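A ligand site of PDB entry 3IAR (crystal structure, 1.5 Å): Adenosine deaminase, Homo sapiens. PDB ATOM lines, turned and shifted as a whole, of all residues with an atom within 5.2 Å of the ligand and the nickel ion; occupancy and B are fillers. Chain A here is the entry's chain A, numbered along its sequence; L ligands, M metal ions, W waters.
An oxygen (O3) of the ligand lies within hydrogen-bond range of the side-chain carboxylate (OD2) of Asp 16 (2.6 Å).
N3 of the ligand lies within hydrogen-bond range of OE1 of Glu 214.
N5 of the ligand sits at hydrogen-bond distance from OD2 of Asp 293 (2.8 Å).
A ring nitrogen (NE2) of His 235 lies close to a nitrogen (N4) of the ligand, at 2.9 Å.
The backbone NH (N) of Gly 181 sits at hydrogen-bond distance from a nitrogen (N2) of the ligand, 3.1 Å away.
The guanidinium group of Arg 98 lies close to a ring nitrogen (ND1) of His 12 (3.4 Å).
The side-chain carboxylate of Asp 292 sits close to a ring nitrogen (NE2) of His 235 (3.1 Å).
OD2 of Asp 292 is in hydrogen-bond range of OG of Ser 262, 2.7 Å away.
OE2 of Glu 214 lies within hydrogen-bond range of NE2 of His 235 (3.2 Å).
N of Leu 103 lies within hydrogen-bond range of OG of Ser 100, 3.2 Å away.
N of Cys 150 is in hydrogen-bond range of O of Tyr 99, at 2.8 Å.
Phe 58 touches the ligand (CZ to N5, 3.9 Å).
CD2 of Leu 59 touches C3 of the ligand, at 3.6 Å.
CE1 of Phe 62 touches O3 of the ligand (3.6 Å).
CA of Tyr 99 touches O1 of the ligand, 3.8 Å away.
Ser 100 touches the ligand.
CD1 of Leu 103 touches O3 of the ligand, at 3.6 Å.
Met 152 touches the ligand.
CB of Ala 180 touches O2 of the ligand (3.7 Å).
Of the 23 residues printed, 17 come within 4 Å of the ligand.
The nearest printed residue that does not touch the ligand is Arg 98 (4.2 Å).
NE2 of His 235 touches the nickel ion, at 3.8 Å.
Within 4 Å of the nickel ion: His 12, His 14, His 211, His 235 and Asp 292.
The nearest printed residue that does not touch the nickel ion is Asp 293 (4.3 Å).
The nickel ion is bound by NE2 of His 14 (2.0 Å), NE2 of His 12 (2.1 Å), OD1 of Asp 292 (2.1 Å), N4 of the ligand (2.2 Å) and NE2 of His 211 (2.2 Å).
Water W1 lies within hydrogen-bond range of OE2 of Glu 214 and OD2 of Asp 292.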
ATOM      1  N   HIS A  12      28.331  -9.931 -16.063  1.00  0.00           N
ATOM      2  CA  HIS A  12      28.008  -8.699 -16.805  1.00  0.00           C
ATOM      3  C   HIS A  12      28.266  -7.483 -15.905  1.00  0.00           C
ATOM      4  O   HIS A  12      27.412  -7.069 -15.114  1.00  0.00           O
ATOM      5  CB  HIS A  12      26.540  -8.712 -17.261  1.00  0.00           C
ATOM      6  CG  HIS A  12      26.218  -7.579 -18.175  1.00  0.00           C
ATOM      7  ND1 HIS A  12      25.800  -7.775 -19.478  1.00  0.00           N
ATOM      8  CD2 HIS A  12      26.333  -6.233 -18.011  1.00  0.00           C
ATOM      9  CE1 HIS A  12      25.603  -6.607 -20.051  1.00  0.00           C
ATOM     10  NE2 HIS A  12      25.953  -5.653 -19.206  1.00  0.00           N
ATOM     11  N   HIS A  14      30.879  -3.800 -16.006  1.00  0.00           N
ATOM     12  CA  HIS A  14      31.814  -3.011 -16.843  1.00  0.00           C
ATOM     13  C   HIS A  14      32.897  -2.405 -15.924  1.00  0.00           C
ATOM     14  O   HIS A  14      32.590  -1.760 -14.911  1.00  0.00           O
ATOM     15  CB  HIS A  14      31.036  -1.861 -17.502  1.00  0.00           C
ATOM     16  CG  HIS A  14      29.979  -2.317 -18.465  1.00  0.00           C
ATOM     17  ND1 HIS A  14      30.075  -2.124 -19.831  1.00  0.00           N
ATOM     18  CD2 HIS A  14      28.768  -2.931 -18.268  1.00  0.00           C
ATOM     19  CE1 HIS A  14      28.986  -2.590 -20.425  1.00  0.00           C
ATOM     20  NE2 HIS A  14      28.176  -3.084 -19.506  1.00  0.00           N
ATOM     21  N   ASP A  16      34.893   0.117 -16.417  1.00  0.00           N
ATOM     22  CA  ASP A  16      34.817   1.580 -16.387  1.00  0.00           C
ATOM     23  C   ASP A  16      33.540   2.105 -15.684  1.00  0.00           C
ATOM     24  O   ASP A  16      33.404   3.280 -15.425  1.00  0.00           O
ATOM     25  CB  ASP A  16      35.007   2.204 -17.796  1.00  0.00           C
ATOM     26  CG  ASP A  16      34.078   1.654 -18.864  1.00  0.00           C
ATOM     27  OD1 ASP A  16      33.381   0.635 -18.680  1.00  0.00           O
ATOM     28  OD2 ASP A  16      34.105   2.298 -19.957  1.00  0.00           O
ATOM     29  N   LEU A  55      18.766   5.392 -21.273  1.00  0.00           N
ATOM     30  CA  LEU A  55      20.107   4.838 -21.515  1.00  0.00           C
ATOM     31  C   LEU A  55      21.112   5.948 -21.934  1.00  0.00           C
ATOM     32  O   LEU A  55      22.237   6.006 -21.440  1.00  0.00           O
ATOM     33  CB  LEU A  55      20.052   3.675 -22.537  1.00  0.00           C
ATOM     34  CG  LEU A  55      21.371   2.931 -22.764  1.00  0.00           C
ATOM     35  CD1 LEU A  55      21.793   2.255 -21.476  1.00  0.00           C
ATOM     36  CD2 LEU A  55      21.264   1.885 -23.896  1.00  0.00           C
ATOM     37  N   PHE A  58      22.140   7.858 -18.826  1.00  0.00           N
ATOM     38  CA  PHE A  58      23.095   7.000 -18.135  1.00  0.00           C
ATOM     39  C   PHE A  58      24.500   7.050 -18.757  1.00  0.00           C
ATOM     40  O   PHE A  58      25.510   7.238 -18.056  1.00  0.00           O
ATOM     41  CB  PHE A  58      22.551   5.561 -18.062  1.00  0.00           C
ATOM     42  CG  PHE A  58      23.613   4.531 -17.893  1.00  0.00           C
ATOM     43  CD1 PHE A  58      24.258   4.366 -16.693  1.00  0.00           C
ATOM     44  CD2 PHE A  58      24.013   3.749 -18.985  1.00  0.00           C
ATOM     45  CE1 PHE A  58      25.253   3.451 -16.549  1.00  0.00           C
ATOM     46  CE2 PHE A  58      25.006   2.806 -18.852  1.00  0.00           C
ATOM     47  CZ  PHE A  58      25.639   2.644 -17.631  1.00  0.00           C
ATOM     48  N   LEU A  59      24.568   6.884 -20.078  1.00  0.00           N
ATOM     49  CA  LEU A  59      25.877   6.825 -20.741  1.00  0.00           C
ATOM     50  C   LEU A  59      26.645   8.121 -20.581  1.00  0.00           C
ATOM     51  O   LEU A  59      27.882   8.103 -20.575  1.00  0.00           O
ATOM     52  CB  LEU A  59      25.707   6.514 -22.235  1.00  0.00           C
ATOM     53  CG  LEU A  59      25.220   5.067 -22.451  1.00  0.00           C
ATOM     54  CD1 LEU A  59      24.765   4.844 -23.899  1.00  0.00           C
ATOM     55  CD2 LEU A  59      26.357   4.097 -22.126  1.00  0.00           C
ATOM     56  N   PHE A  62      29.539   8.847 -17.750  1.00  0.00           N
ATOM     57  CA  PHE A  62      30.941   8.496 -17.926  1.00  0.00           C
ATOM     58  C   PHE A  62      31.803   9.724 -18.204  1.00  0.00           C
ATOM     59  O   PHE A  62      33.009   9.734 -17.855  1.00  0.00           O
ATOM     60  CB  PHE A  62      31.081   7.478 -19.089  1.00  0.00           C
ATOM     61  CG  PHE A  62      30.611   6.107 -18.724  1.00  0.00           C
ATOM     62  CD1 PHE A  62      31.531   5.150 -18.316  1.00  0.00           C
ATOM     63  CD2 PHE A  62      29.244   5.787 -18.747  1.00  0.00           C
ATOM     64  CE1 PHE A  62      31.090   3.870 -17.960  1.00  0.00           C
ATOM     65  CE2 PHE A  62      28.834   4.531 -18.376  1.00  0.00           C
ATOM     66  CZ  PHE A  62      29.753   3.582 -17.980  1.00  0.00           C
ATOM     67  N   MET A  66      35.690   9.633 -16.635  1.00  0.00           N
ATOM     68  CA  MET A  66      36.626   8.904 -17.473  1.00  0.00           C
ATOM     69  C   MET A  66      37.885   9.721 -17.853  1.00  0.00           C
ATOM     70  O   MET A  66      38.963   9.134 -17.955  1.00  0.00           O
ATOM     71  CB  MET A  66      35.939   8.367 -18.729  1.00  0.00           C
ATOM     72  CG  MET A  66      34.975   7.208 -18.488  1.00  0.00           C
ATOM     73  SD  MET A  66      35.907   5.717 -18.014  1.00  0.00           S
ATOM     74  CE  MET A  66      36.368   5.162 -19.681  1.00  0.00           C
ATOM     75  N   ARG A  98      34.073  -6.473 -18.232  1.00  0.00           N
ATOM     76  CA  ARG A  98      34.122  -6.010 -19.637  1.00  0.00           C
ATOM     77  C   ARG A  98      34.449  -4.520 -19.714  1.00  0.00           C
ATOM     78  O   ARG A  98      34.171  -3.740 -18.808  1.00  0.00           O
ATOM     79  CB  ARG A  98      32.783  -6.310 -20.360  1.00  0.00           C
ATOM     80  CG  ARG A  98      31.603  -5.507 -19.888  1.00  0.00           C
ATOM     81  CD  ARG A  98      30.335  -6.075 -20.562  1.00  0.00           C
ATOM     82  NE  ARG A  98      30.069  -7.449 -20.185  1.00  0.00           N
ATOM     83  CZ  ARG A  98      29.091  -8.184 -20.737  1.00  0.00           C
ATOM     84  NH1 ARG A  98      28.357  -7.642 -21.724  1.00  0.00           N
ATOM     85  NH2 ARG A  98      28.854  -9.416 -20.306  1.00  0.00           N
ATOM     86  N   TYR A  99      35.068  -4.133 -20.829  1.00  0.00           N
ATOM     87  CA  TYR A  99      35.400  -2.721 -21.056  1.00  0.00           C
ATOM     88  C   TYR A  99      35.803  -2.523 -22.508  1.00  0.00           C
ATOM     89  O   TYR A  99      36.115  -3.503 -23.228  1.00  0.00           O
ATOM     90  CB  TYR A  99      36.560  -2.256 -20.131  1.00  0.00           C
ATOM     91  CG  TYR A  99      37.857  -2.961 -20.415  1.00  0.00           C
ATOM     92  CD1 TYR A  99      38.835  -2.364 -21.209  1.00  0.00           C
ATOM     93  CD2 TYR A  99      38.073  -4.273 -19.954  1.00  0.00           C
ATOM     94  CE1 TYR A  99      40.026  -3.025 -21.504  1.00  0.00           C
ATOM     95  CE2 TYR A  99      39.261  -4.948 -20.259  1.00  0.00           C
ATOM     96  CZ  TYR A  99      40.232  -4.307 -21.073  1.00  0.00           C
ATOM     97  OH  TYR A  99      41.409  -4.942 -21.357  1.00  0.00           O
ATOM     98  N   SER A 100      35.771  -1.274 -22.954  1.00  0.00           N
ATOM     99  CA  SER A 100      36.319  -0.886 -24.252  1.00  0.00           C
ATOM    100  C   SER A 100      37.755  -0.414 -24.069  1.00  0.00           C
ATOM    101  O   SER A 100      37.978   0.608 -23.440  1.00  0.00           O
ATOM    102  CB  SER A 100      35.519   0.303 -24.821  1.00  0.00           C
ATOM    103  OG  SER A 100      36.214   0.871 -25.928  1.00  0.00           O
ATOM    104  N   LEU A 103      38.312   3.183 -25.200  1.00  0.00           N
ATOM    105  CA  LEU A 103      37.852   4.281 -24.348  1.00  0.00           C
ATOM    106  C   LEU A 103      38.829   4.601 -23.204  1.00  0.00           C
ATOM    107  O   LEU A 103      38.633   5.583 -22.494  1.00  0.00           O
ATOM    108  CB  LEU A 103      36.439   4.016 -23.807  1.00  0.00           C
ATOM    109  CG  LEU A 103      35.401   4.034 -24.907  1.00  0.00           C
ATOM    110  CD1 LEU A 103      34.052   3.687 -24.240  1.00  0.00           C
ATOM    111  CD2 LEU A 103      35.350   5.371 -25.549  1.00  0.00           C
ATOM    112  N   CYS A 150      34.861  -4.891 -25.271  1.00  0.00           N
ATOM    113  CA  CYS A 150      33.669  -4.354 -25.938  1.00  0.00           C
ATOM    114  C   CYS A 150      33.935  -3.635 -27.254  1.00  0.00           C
ATOM    115  O   CYS A 150      34.670  -2.634 -27.281  1.00  0.00           O
ATOM    116  CB  CYS A 150      32.968  -3.330 -25.011  1.00  0.00           C
ATOM    117  SG  CYS A 150      32.468  -3.985 -23.403  1.00  0.00           S
ATOM    118  N   MET A 152      31.941  -1.047 -29.576  1.00  0.00           N
ATOM    119  CA  MET A 152      30.946  -0.027 -29.238  1.00  0.00           C
ATOM    120  C   MET A 152      30.069   0.267 -30.455  1.00  0.00           C
ATOM    121  O   MET A 152      30.603   0.413 -31.558  1.00  0.00           O
ATOM    122  CB  MET A 152      31.658   1.265 -28.815  1.00  0.00           C
ATOM    123  CG  MET A 152      32.502   1.093 -27.501  1.00  0.00           C
ATOM    124  SD  MET A 152      31.551   0.449 -26.109  1.00  0.00           S
ATOM    125  CE  MET A 152      30.452   1.822 -25.868  1.00  0.00           C
ATOM    126  N   ALA A 180      28.509  -3.105 -26.968  1.00  0.00           N
ATOM    127  CA  ALA A 180      27.862  -2.266 -25.994  1.00  0.00           C
ATOM    128  C   ALA A 180      27.602  -0.886 -26.620  1.00  0.00           C
ATOM    129  O   ALA A 180      27.866  -0.681 -27.811  1.00  0.00           O
ATOM    130  CB  ALA A 180      28.705  -2.165 -24.678  1.00  0.00           C
ATOM    131  N   GLY A 181      27.122   0.048 -25.803  1.00  0.00           N
ATOM    132  CA  GLY A 181      26.798   1.384 -26.297  1.00  0.00           C
ATOM    133  C   GLY A 181      25.302   1.547 -26.523  1.00  0.00           C
ATOM    134  O   GLY A 181      24.466   0.798 -25.979  1.00  0.00           O
ATOM    135  N   ASP A 182      24.959   2.527 -27.361  1.00  0.00           N
ATOM    136  CA  ASP A 182      23.553   2.896 -27.528  1.00  0.00           C
ATOM    137  C   ASP A 182      22.842   1.980 -28.520  1.00  0.00           C
ATOM    138  O   ASP A 182      22.995   2.051 -29.742  1.00  0.00           O
ATOM    139  CB  ASP A 182      23.466   4.385 -27.946  1.00  0.00           C
ATOM    140  CG  ASP A 182      22.016   4.813 -28.267  1.00  0.00           C
ATOM    141  OD1 ASP A 182      21.095   3.984 -28.119  1.00  0.00           O
ATOM    142  OD2 ASP A 182      21.826   5.975 -28.697  1.00  0.00           O
ATOM    143  N   HIS A 211      25.136  -6.910 -25.959  1.00  0.00           N
ATOM    144  CA  HIS A 211      24.065  -6.183 -25.283  1.00  0.00           C
ATOM    145  C   HIS A 211      22.892  -6.066 -26.249  1.00  0.00           C
ATOM    146  O   HIS A 211      23.044  -5.444 -27.309  1.00  0.00           O
ATOM    147  CB  HIS A 211      24.516  -4.774 -24.943  1.00  0.00           C
ATOM    148  CG  HIS A 211      25.370  -4.623 -23.697  1.00  0.00           C
ATOM    149  ND1 HIS A 211      26.722  -4.975 -23.626  1.00  0.00           N
ATOM    150  CD2 HIS A 211      25.081  -4.014 -22.512  1.00  0.00           C
ATOM    151  CE1 HIS A 211      27.189  -4.633 -22.433  1.00  0.00           C
ATOM    152  NE2 HIS A 211      26.223  -4.037 -21.746  1.00  0.00           N
ATOM    153  N   GLU A 214      17.937  -4.531 -24.131  1.00  0.00           N
ATOM    154  CA  GLU A 214      18.015  -3.787 -22.878  1.00  0.00           C
ATOM    155  C   GLU A 214      16.992  -2.705 -23.014  1.00  0.00           C
ATOM    156  O   GLU A 214      16.016  -2.648 -22.246  1.00  0.00           O
ATOM    157  CB  GLU A 214      19.405  -3.195 -22.675  1.00  0.00           C
ATOM    158  CG  GLU A 214      19.550  -2.300 -21.409  1.00  0.00           C
ATOM    159  CD  GLU A 214      20.944  -1.737 -21.270  1.00  0.00           C
ATOM    160  OE1 GLU A 214      21.822  -1.892 -22.202  1.00  0.00           O
ATOM    161  OE2 GLU A 214      21.233  -1.104 -20.220  1.00  0.00           O
ATOM    162  N   HIS A 235      21.517  -8.330 -20.821  1.00  0.00           N
ATOM    163  CA  HIS A 235      20.169  -7.856 -20.512  1.00  0.00           C
ATOM    164  C   HIS A 235      19.113  -8.757 -21.156  1.00  0.00           C
ATOM    165  O   HIS A 235      18.641  -9.703 -20.518  1.00  0.00           O
ATOM    166  CB  HIS A 235      19.987  -6.354 -20.886  1.00  0.00           C
ATOM    167  CG  HIS A 235      20.917  -5.428 -20.152  1.00  0.00           C
ATOM    168  ND1 HIS A 235      20.756  -5.125 -18.813  1.00  0.00           N
ATOM    169  CD2 HIS A 235      21.981  -4.725 -20.577  1.00  0.00           C
ATOM    170  CE1 HIS A 235      21.698  -4.263 -18.446  1.00  0.00           C
ATOM    171  NE2 HIS A 235      22.458  -4.014 -19.490  1.00  0.00           N
ATOM    172  N   SER A 262      20.209  -2.187 -12.417  1.00  0.00           N
ATOM    173  CA  SER A 262      20.542  -1.449 -13.622  1.00  0.00           C
ATOM    174  C   SER A 262      19.297  -1.222 -14.486  1.00  0.00           C
ATOM    175  O   SER A 262      19.056  -0.118 -14.978  1.00  0.00           O
ATOM    176  CB  SER A 262      21.572  -2.269 -14.429  1.00  0.00           C
ATOM    177  OG  SER A 262      21.704  -1.726 -15.734  1.00  0.00           O
ATOM    178  N   ASP A 292      26.262  -4.692 -13.590  1.00  0.00           N
ATOM    179  CA  ASP A 292      26.396  -3.851 -14.798  1.00  0.00           C
ATOM    180  C   ASP A 292      27.329  -2.659 -14.597  1.00  0.00           C
ATOM    181  O   ASP A 292      28.508  -2.695 -15.006  1.00  0.00           O
ATOM    182  CB  ASP A 292      24.972  -3.444 -15.310  1.00  0.00           C
ATOM    183  CG  ASP A 292      24.952  -2.995 -16.752  1.00  0.00           C
ATOM    184  OD1 ASP A 292      25.928  -3.268 -17.508  1.00  0.00           O
ATOM    185  OD2 ASP A 292      23.882  -2.444 -17.163  1.00  0.00           O
ATOM    186  N   ASP A 293      26.850  -1.603 -13.929  1.00  0.00           N
ATOM    187  CA  ASP A 293      27.667  -0.407 -13.705  1.00  0.00           C
ATOM    188  C   ASP A 293      27.492   0.093 -12.269  1.00  0.00           C
ATOM    189  O   ASP A 293      26.922   1.156 -12.030  1.00  0.00           O
ATOM    190  CB  ASP A 293      27.311   0.709 -14.706  1.00  0.00           C
ATOM    191  CG  ASP A 293      27.604   0.289 -16.141  1.00  0.00           C
ATOM    192  OD1 ASP A 293      28.740   0.489 -16.605  1.00  0.00           O
ATOM    193  OD2 ASP A 293      26.720  -0.362 -16.772  1.00  0.00           O
HETATM  194  O1  LIG L   1      32.237  -0.579 -20.742  1.00  0.00           O
HETATM  195  C1  LIG L   1      32.353   0.039 -22.035  1.00  0.00           C
HETATM  196  C2  LIG L   1      31.282   1.092 -22.309  1.00  0.00           C
HETATM  197  O2  LIG L   1      29.947   0.481 -22.392  1.00  0.00           O
HETATM  198  C3  LIG L   1      28.909   1.522 -22.122  1.00  0.00           C
HETATM  199  N1  LIG L   1      28.006   0.757 -21.271  1.00  0.00           N
HETATM  200  C4  LIG L   1      26.808   0.196 -21.688  1.00  0.00           C
HETATM  201  N2  LIG L   1      26.207   0.338 -22.882  1.00  0.00           N
HETATM  202  C5  LIG L   1      25.044  -0.297 -22.929  1.00  0.00           C
HETATM  203  N3  LIG L   1      24.476  -1.030 -21.950  1.00  0.00           N
HETATM  204  C6  LIG L   1      25.149  -1.233 -20.771  1.00  0.00           C
HETATM  205  N4  LIG L   1      24.675  -2.110 -19.884  1.00  0.00           N
HETATM  206  C7  LIG L   1      26.366  -0.517 -20.602  1.00  0.00           C
HETATM  207  N5  LIG L   1      27.238  -0.426 -19.530  1.00  0.00           N
HETATM  208  C8  LIG L   1      28.207   0.344 -19.959  1.00  0.00           C
HETATM  209  C9  LIG L   1      29.644   2.685 -21.506  1.00  0.00           C
HETATM  210  C10 LIG L   1      31.077   2.157 -21.210  1.00  0.00           C
HETATM  211  O3  LIG L   1      32.029   3.194 -21.319  1.00  0.00           O
HETATM  212 NI    NI M   1      26.200  -3.601 -19.581  1.00  0.00          NI
HETATM  213  O   HOH W   1      23.299  -0.014 -18.666  1.00  0.00           O
HETATM  214  O   HOH W   2      31.532   5.598 -22.650  1.00  0.00           O
